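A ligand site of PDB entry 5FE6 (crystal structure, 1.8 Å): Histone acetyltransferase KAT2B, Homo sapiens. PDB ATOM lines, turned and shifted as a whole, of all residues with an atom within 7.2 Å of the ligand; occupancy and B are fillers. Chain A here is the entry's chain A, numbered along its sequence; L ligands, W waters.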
ATOM      1  N   TRP A  34     -21.166  12.350  12.868  1.00  0.00           N
ATOM      2  CA  TRP A  34     -19.757  12.675  12.734  1.00  0.00           C
ATOM      3  C   TRP A  34     -19.420  14.162  12.977  1.00  0.00           C
ATOM      4  O   TRP A  34     -18.336  14.451  13.515  1.00  0.00           O
ATOM      5  CB  TRP A  34     -19.161  12.178  11.389  1.00  0.00           C
ATOM      6  CG  TRP A  34     -19.669  12.842  10.159  1.00  0.00           C
ATOM      7  CD1 TRP A  34     -20.694  12.445   9.386  1.00  0.00           C
ATOM      8  CD2 TRP A  34     -19.200  14.097   9.596  1.00  0.00           C
ATOM      9  NE1 TRP A  34     -20.881  13.339   8.378  1.00  0.00           N
ATOM     10  CE2 TRP A  34     -19.972  14.350   8.493  1.00  0.00           C
ATOM     11  CE3 TRP A  34     -18.194  15.001   9.956  1.00  0.00           C
ATOM     12  CZ2 TRP A  34     -19.809  15.505   7.702  1.00  0.00           C
ATOM     13  CZ3 TRP A  34     -18.052  16.161   9.187  1.00  0.00           C
ATOM     14  CH2 TRP A  34     -18.822  16.365   8.079  1.00  0.00           C
ATOM     15  N   PRO A  35     -20.309  15.083  12.600  1.00  0.00           N
ATOM     16  CA  PRO A  35     -19.961  16.486  12.861  1.00  0.00           C
ATOM     17  C   PRO A  35     -20.003  16.921  14.324  1.00  0.00           C
ATOM     18  O   PRO A  35     -19.488  17.990  14.658  1.00  0.00           O
ATOM     19  CB  PRO A  35     -21.040  17.287  12.119  1.00  0.00           C
ATOM     20  CG  PRO A  35     -21.693  16.324  11.164  1.00  0.00           C
ATOM     21  CD  PRO A  35     -21.574  14.976  11.816  1.00  0.00           C
ATOM     22  N   PHE A  36     -20.612  16.115  15.170  1.00  0.00           N
ATOM     23  CA  PHE A  36     -20.975  16.493  16.496  1.00  0.00           C
ATOM     24  C   PHE A  36     -20.219  15.716  17.534  1.00  0.00           C
ATOM     25  O   PHE A  36     -20.492  15.827  18.713  1.00  0.00           O
ATOM     26  CB  PHE A  36     -22.506  16.245  16.697  1.00  0.00           C
ATOM     27  CG  PHE A  36     -23.352  16.838  15.619  1.00  0.00           C
ATOM     28  CD1 PHE A  36     -23.397  18.213  15.412  1.00  0.00           C
ATOM     29  CD2 PHE A  36     -24.032  16.014  14.772  1.00  0.00           C
ATOM     30  CE1 PHE A  36     -24.072  18.758  14.325  1.00  0.00           C
ATOM     31  CE2 PHE A  36     -24.758  16.530  13.714  1.00  0.00           C
ATOM     32  CZ  PHE A  36     -24.775  17.917  13.479  1.00  0.00           C
ATOM     33  N   MET A  37     -19.219  14.973  17.096  1.00  0.00           N
ATOM     34  CA  MET A  37     -18.574  13.981  17.990  1.00  0.00           C
ATOM     35  C   MET A  37     -17.690  14.641  19.083  1.00  0.00           C
ATOM     36  O   MET A  37     -17.571  14.067  20.191  1.00  0.00           O
ATOM     37  CB  MET A  37     -17.779  12.987  17.159  1.00  0.00           C
ATOM     38  CG  MET A  37     -18.605  12.051  16.311  1.00  0.00           C
ATOM     39  SD  MET A  37     -19.676  10.985  17.240  1.00  0.00           S
ATOM     40  CE  MET A  37     -18.484   9.921  18.008  1.00  0.00           C
ATOM     41  N   GLU A  38     -17.083  15.795  18.788  1.00  0.00           N
ATOM     42  CA  GLU A  38     -16.145  16.467  19.697  1.00  0.00           C
ATOM     43  C   GLU A  38     -16.370  17.949  19.585  1.00  0.00           C
ATOM     44  O   GLU A  38     -17.029  18.389  18.626  1.00  0.00           O
ATOM     45  CB  GLU A  38     -14.668  16.101  19.327  1.00  0.00           C
ATOM     46  CG  GLU A  38     -14.443  14.632  19.352  1.00  0.00           C
ATOM     47  CD  GLU A  38     -12.990  14.188  19.409  1.00  0.00           C
ATOM     48  OE1 GLU A  38     -12.147  14.827  18.746  1.00  0.00           O
ATOM     49  OE2 GLU A  38     -12.747  13.178  20.107  1.00  0.00           O
ATOM     50  N   PRO A  39     -15.840  18.746  20.528  1.00  0.00           N
ATOM     51  CA  PRO A  39     -16.021  20.205  20.423  1.00  0.00           C
ATOM     52  C   PRO A  39     -15.584  20.742  19.068  1.00  0.00           C
ATOM     53  O   PRO A  39     -14.594  20.282  18.473  1.00  0.00           O
ATOM     54  CB  PRO A  39     -15.123  20.753  21.551  1.00  0.00           C
ATOM     55  CG  PRO A  39     -15.118  19.643  22.558  1.00  0.00           C
ATOM     56  CD  PRO A  39     -15.106  18.368  21.765  1.00  0.00           C
ATOM     57  N   VAL A  40     -16.347  21.686  18.543  1.00  0.00           N
ATOM     58  CA  VAL A  40     -15.987  22.357  17.296  1.00  0.00           C
ATOM     59  C   VAL A  40     -14.543  22.889  17.393  1.00  0.00           C
ATOM     60  O   VAL A  40     -14.151  23.413  18.439  1.00  0.00           O
ATOM     61  CB  VAL A  40     -17.013  23.468  16.934  1.00  0.00           C
ATOM     62  CG1 VAL A  40     -16.560  24.308  15.762  1.00  0.00           C
ATOM     63  CG2 VAL A  40     -18.365  22.818  16.597  1.00  0.00           C
ATOM     64  N   LYS A  41     -13.793  22.678  16.336  1.00  0.00           N
ATOM     65  CA  LYS A  41     -12.372  23.056  16.283  1.00  0.00           C
ATOM     66  C   LYS A  41     -12.263  24.455  15.669  1.00  0.00           C
ATOM     67  O   LYS A  41     -12.854  24.725  14.637  1.00  0.00           O
ATOM     68  CB  LYS A  41     -11.575  22.047  15.435  1.00  0.00           C
ATOM     69  CG  LYS A  41     -11.230  20.729  16.119  1.00  0.00           C
ATOM     70  CD  LYS A  41     -10.356  19.794  15.271  1.00  0.00           C
ATOM     71  CE  LYS A  41      -9.070  20.458  14.845  1.00  0.00           C
ATOM     72  NZ  LYS A  41      -8.031  19.526  14.271  1.00  0.00           N
ATOM     73  N   GLU A  44     -11.360  24.720  12.134  1.00  0.00           N
ATOM     74  CA  GLU A  44     -12.385  24.499  11.111  1.00  0.00           C
ATOM     75  C   GLU A  44     -13.446  25.629  11.037  1.00  0.00           C
ATOM     76  O   GLU A  44     -14.081  25.865  10.004  1.00  0.00           O
ATOM     77  CB  GLU A  44     -13.006  23.086  11.338  1.00  0.00           C
ATOM     78  CG  GLU A  44     -11.988  21.943  11.365  1.00  0.00           C
ATOM     79  CD  GLU A  44     -12.555  20.597  11.875  1.00  0.00           C
ATOM     80  OE1 GLU A  44     -13.664  20.585  12.391  1.00  0.00           O
ATOM     81  OE2 GLU A  44     -11.873  19.544  11.770  1.00  0.00           O
ATOM     82  N   ALA A  45     -13.535  26.433  12.092  1.00  0.00           N
ATOM     83  CA  ALA A  45     -14.559  27.420  12.222  1.00  0.00           C
ATOM     84  C   ALA A  45     -14.007  28.597  13.035  1.00  0.00           C
ATOM     85  O   ALA A  45     -14.376  28.787  14.195  1.00  0.00           O
ATOM     86  CB  ALA A  45     -15.732  26.781  12.938  1.00  0.00           C
ATOM     87  N   PRO A  46     -13.099  29.395  12.441  1.00  0.00           N
ATOM     88  CA  PRO A  46     -12.304  30.291  13.271  1.00  0.00           C
ATOM     89  C   PRO A  46     -13.084  31.217  14.218  1.00  0.00           C
ATOM     90  O   PRO A  46     -12.628  31.472  15.308  1.00  0.00           O
ATOM     91  CB  PRO A  46     -11.480  31.074  12.237  1.00  0.00           C
ATOM     92  CG  PRO A  46     -11.271  30.057  11.139  1.00  0.00           C
ATOM     93  CD  PRO A  46     -12.539  29.271  11.075  1.00  0.00           C
ATOM     94  N   TYR A  48     -16.171  30.689  15.422  1.00  0.00           N
ATOM     95  CA  TYR A  48     -17.291  29.935  16.053  1.00  0.00           C
ATOM     96  C   TYR A  48     -17.592  30.336  17.455  1.00  0.00           C
ATOM     97  O   TYR A  48     -18.748  30.573  17.842  1.00  0.00           O
ATOM     98  CB  TYR A  48     -16.967  28.429  16.022  1.00  0.00           C
ATOM     99  CG  TYR A  48     -18.126  27.554  16.434  1.00  0.00           C
ATOM    100  CD1 TYR A  48     -19.069  27.145  15.512  1.00  0.00           C
ATOM    101  CD2 TYR A  48     -18.284  27.131  17.751  1.00  0.00           C
ATOM    102  CE1 TYR A  48     -20.124  26.297  15.867  1.00  0.00           C
ATOM    103  CE2 TYR A  48     -19.345  26.326  18.106  1.00  0.00           C
ATOM    104  CZ  TYR A  48     -20.267  25.912  17.161  1.00  0.00           C
ATOM    105  OH  TYR A  48     -21.342  25.090  17.545  1.00  0.00           O
ATOM    106  N   ILE A  52     -21.233  31.271  18.970  1.00  0.00           N
ATOM    107  CA  ILE A  52     -21.965  30.277  19.729  1.00  0.00           C
ATOM    108  C   ILE A  52     -21.570  30.327  21.172  1.00  0.00           C
ATOM    109  O   ILE A  52     -20.461  29.933  21.536  1.00  0.00           O
ATOM    110  CB  ILE A  52     -21.682  28.925  19.136  1.00  0.00           C
ATOM    111  CG1 ILE A  52     -22.164  28.906  17.681  1.00  0.00           C
ATOM    112  CG2 ILE A  52     -22.289  27.790  19.962  1.00  0.00           C
ATOM    113  CD1 ILE A  52     -23.661  29.002  17.515  1.00  0.00           C
ATOM    114  N   MET A  56     -21.819  22.683  22.545  1.00  0.00           N
ATOM    115  CA  MET A  56     -22.072  21.357  23.088  1.00  0.00           C
ATOM    116  C   MET A  56     -21.770  20.345  22.002  1.00  0.00           C
ATOM    117  O   MET A  56     -21.913  20.637  20.825  1.00  0.00           O
ATOM    118  CB  MET A  56     -23.539  21.219  23.577  1.00  0.00           C
ATOM    119  CG  MET A  56     -23.887  19.968  24.332  1.00  0.00           C
ATOM    120  SD  MET A  56     -22.775  19.490  25.672  1.00  0.00           S
ATOM    121  CE  MET A  56     -22.849  20.937  26.689  1.00  0.00           C
ATOM    122  N   VAL A  83     -26.887  20.829  20.815  1.00  0.00           N
ATOM    123  CA  VAL A  83     -25.981  20.460  19.709  1.00  0.00           C
ATOM    124  C   VAL A  83     -26.660  20.837  18.393  1.00  0.00           C
ATOM    125  O   VAL A  83     -26.060  21.435  17.478  1.00  0.00           O
ATOM    126  CB  VAL A  83     -25.725  18.939  19.770  1.00  0.00           C
ATOM    127  CG1 VAL A  83     -25.010  18.508  18.501  1.00  0.00           C
ATOM    128  CG2 VAL A  83     -24.949  18.552  21.013  1.00  0.00           C
ATOM    129  N   ASN A  86     -27.283  24.818  18.016  1.00  0.00           N
ATOM    130  CA  ASN A  86     -26.007  25.459  17.641  1.00  0.00           C
ATOM    131  C   ASN A  86     -25.744  25.259  16.151  1.00  0.00           C
ATOM    132  O   ASN A  86     -25.348  26.203  15.445  1.00  0.00           O
ATOM    133  CB  ASN A  86     -24.825  24.907  18.435  1.00  0.00           C
ATOM    134  CG  ASN A  86     -24.860  25.322  19.887  1.00  0.00           C
ATOM    135  OD1 ASN A  86     -25.618  26.224  20.280  1.00  0.00           O
ATOM    136  ND2 ASN A  86     -24.054  24.678  20.705  1.00  0.00           N
ATOM    137  N   CYS A  87     -25.943  24.023  15.678  1.00  0.00           N
ATOM    138  CA  CYS A  87     -25.652  23.693  14.310  1.00  0.00           C
ATOM    139  C   CYS A  87     -26.517  24.542  13.374  1.00  0.00           C
ATOM    140  O   CYS A  87     -26.041  25.058  12.372  1.00  0.00           O
ATOM    141  CB  CYS A  87     -25.814  22.186  14.070  1.00  0.00           C
ATOM    142  SG  CYS A  87     -25.515  21.697  12.351  1.00  0.00           S
ATOM    143  N   LYS A  88     -27.817  24.631  13.685  1.00  0.00           N
ATOM    144  CA  LYS A  88     -28.756  25.342  12.795  1.00  0.00           C
ATOM    145  C   LYS A  88     -28.566  26.873  12.885  1.00  0.00           C
ATOM    146  O   LYS A  88     -28.843  27.605  11.929  1.00  0.00           O
ATOM    147  CB  LYS A  88     -30.155  24.899  13.132  1.00  0.00           C
ATOM    148  CG  LYS A  88     -30.425  23.463  12.855  1.00  0.00           C
ATOM    149  CD  LYS A  88     -31.727  23.006  13.418  1.00  0.00           C
ATOM    150  CE  LYS A  88     -32.019  21.588  13.026  1.00  0.00           C
ATOM    151  NZ  LYS A  88     -33.209  21.053  13.666  1.00  0.00           N
ATOM    152  N   TYR A  90     -25.580  28.237  13.378  1.00  0.00           N
ATOM    153  CA  TYR A  90     -24.349  28.556  12.740  1.00  0.00           C
ATOM    154  C   TYR A  90     -24.306  28.341  11.229  1.00  0.00           C
ATOM    155  O   TYR A  90     -23.644  29.135  10.528  1.00  0.00           O
ATOM    156  CB  TYR A  90     -23.194  27.807  13.442  1.00  0.00           C
ATOM    157  CG  TYR A  90     -21.860  28.407  13.161  1.00  0.00           C
ATOM    158  CD1 TYR A  90     -21.439  29.559  13.834  1.00  0.00           C
ATOM    159  CD2 TYR A  90     -21.001  27.841  12.218  1.00  0.00           C
ATOM    160  CE1 TYR A  90     -20.219  30.179  13.535  1.00  0.00           C
ATOM    161  CE2 TYR A  90     -19.758  28.442  11.913  1.00  0.00           C
ATOM    162  CZ  TYR A  90     -19.378  29.603  12.563  1.00  0.00           C
ATOM    163  OH  TYR A  90     -18.157  30.210  12.315  1.00  0.00           O
ATOM    164  N   ASN A  91     -24.931  27.279  10.737  1.00  0.00           N
ATOM    165  CA  ASN A  91     -24.757  26.797   9.386  1.00  0.00           C
ATOM    166  C   ASN A  91     -26.021  27.038   8.524  1.00  0.00           C
ATOM    167  O   ASN A  91     -27.148  26.981   9.041  1.00  0.00           O
ATOM    168  CB  ASN A  91     -24.452  25.318   9.383  1.00  0.00           C
ATOM    169  CG  ASN A  91     -23.218  25.001  10.153  1.00  0.00           C
ATOM    170  OD1 ASN A  91     -22.113  25.320   9.686  1.00  0.00           O
ATOM    171  ND2 ASN A  91     -23.363  24.458  11.327  1.00  0.00           N
ATOM    172  N   TYR A  97     -23.907  19.895   7.362  1.00  0.00           N
ATOM    173  CA  TYR A  97     -24.073  19.886   8.832  1.00  0.00           C
ATOM    174  C   TYR A  97     -25.534  19.998   9.250  1.00  0.00           C
ATOM    175  O   TYR A  97     -25.997  19.268  10.144  1.00  0.00           O
ATOM    176  CB  TYR A  97     -23.303  21.026   9.475  1.00  0.00           C
ATOM    177  CG  TYR A  97     -21.850  20.992   9.148  1.00  0.00           C
ATOM    178  CD1 TYR A  97     -21.071  19.891   9.421  1.00  0.00           C
ATOM    179  CD2 TYR A  97     -21.264  22.083   8.566  1.00  0.00           C
ATOM    180  CE1 TYR A  97     -19.705  19.867   9.110  1.00  0.00           C
ATOM    181  CE2 TYR A  97     -19.925  22.070   8.255  1.00  0.00           C
ATOM    182  CZ  TYR A  97     -19.172  20.980   8.526  1.00  0.00           C
ATOM    183  OH  TYR A  97     -17.851  21.049   8.186  1.00  0.00           O
ATOM    184  N   TYR A  98     -26.246  20.970   8.662  1.00  0.00           N
ATOM    185  CA  TYR A  98     -27.643  21.139   8.954  1.00  0.00           C
ATOM    186  C   TYR A  98     -28.406  19.860   8.612  1.00  0.00           C
ATOM    187  O   TYR A  98     -29.257  19.392   9.418  1.00  0.00           O
ATOM    188  CB  TYR A  98     -28.164  22.362   8.193  1.00  0.00           C
ATOM    189  CG  TYR A  98     -29.491  22.949   8.679  1.00  0.00           C
ATOM    190  CD1 TYR A  98     -30.661  22.211   8.605  1.00  0.00           C
ATOM    191  CD2 TYR A  98     -29.561  24.257   9.183  1.00  0.00           C
ATOM    192  CE1 TYR A  98     -31.912  22.758   9.035  1.00  0.00           C
ATOM    193  CE2 TYR A  98     -30.784  24.814   9.619  1.00  0.00           C
ATOM    194  CZ  TYR A  98     -31.961  24.061   9.551  1.00  0.00           C
ATOM    195  OH  TYR A  98     -33.263  24.501  10.009  1.00  0.00           O
ATOM    196  N   ALA A 101     -27.770  17.292  11.220  1.00  0.00           N
ATOM    197  CA  ALA A 101     -28.515  17.612  12.426  1.00  0.00           C
ATOM    198  C   ALA A 101     -29.970  17.093  12.387  1.00  0.00           C
ATOM    199  O   ALA A 101     -30.438  16.520  13.337  1.00  0.00           O
ATOM    200  CB  ALA A 101     -28.446  19.100  12.757  1.00  0.00           C
HETATM  201  C1  LIG L   1     -17.148  23.312  10.928  1.00  0.00           C
HETATM  202  C2  LIG L   1     -20.289  22.984  13.007  1.00  0.00           C
HETATM  203  C3  LIG L   1     -20.443  21.567  13.096  1.00  0.00           C
HETATM  204  N1  LIG L   1     -19.139  23.465  12.459  1.00  0.00           N
HETATM  205  C4  LIG L   1     -21.835  21.058  13.219  1.00  0.00           C
HETATM  206  C5  LIG L   1     -20.945  21.035  14.409  1.00  0.00           C
HETATM  207  O1  LIG L   1     -21.228  23.706  13.336  1.00  0.00           O
HETATM  208  C6  LIG L   1     -18.823  24.881  12.286  1.00  0.00           C
HETATM  209  C7  LIG L   1     -18.761  25.268  10.806  1.00  0.00           C
HETATM  210  C8  LIG L   1     -18.064  22.602  11.931  1.00  0.00           C
HETATM  211  C9  LIG L   1     -17.938  24.249  10.027  1.00  0.00           C
HETATM  212  N2  LIG L   1     -17.059  24.890   9.047  1.00  0.00           N
HETATM  213  O   HOH W   1     -16.345  27.356   8.843  1.00  0.00           O
HETATM  214  O   HOH W   2     -18.420  25.439   6.530  1.00  0.00           O
HETATM  215  O   HOH W   3     -22.593  23.918  15.602  1.00  0.00           O
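The side-chain amide nitrogen (ND2) of Asn 91 is in hydrogen-bond range of an oxygen (O1) of the ligand, 3.0 Å away.
N2 of the ligand sits at hydrogen-bond distance from O of Glu 44.
The backbone carbonyl oxygen of Tyr 97 lies within hydrogen-bond range of the side-chain sulfur of Cys 87 (3.3 Å).
ND2 of Asn 91 sits at hydrogen-bond distance from O of Cys 87 (2.9 Å).
Residues that only touch the ligand: Pro 35 (3.4 Å), Phe 36 (3.4 Å), Val 40 (3.8 Å), Ala 45 (3.7 Å), Tyr 48 (3.8 Å), Cys 87 (3.8 Å), Tyr 90 (3.5 Å) and Tyr 97 (3.4 Å).
Hydrophobic or aromatic side chains that line the ligand: Phe 36, Val 40, Ala 45, Tyr 48, Tyr 90 and Tyr 97.
Within 4 Å of the ligand: Pro 35, Phe 36, Val 40, Glu 44, Ala 45, Tyr 48, Cys 87, Tyr 90, Asn 91 and Tyr 97.
Water W1 lies within hydrogen-bond range of N2 of the ligand (2.6 Å) and O of Glu 44 (2.9 Å).
Water W3 lies within hydrogen-bond range of the side-chain hydroxyl of Tyr 48 (2.6 Å), an oxygen (O1) of the ligand (2.7 Å) and the backbone NH of Cys 87 (3.4 Å).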
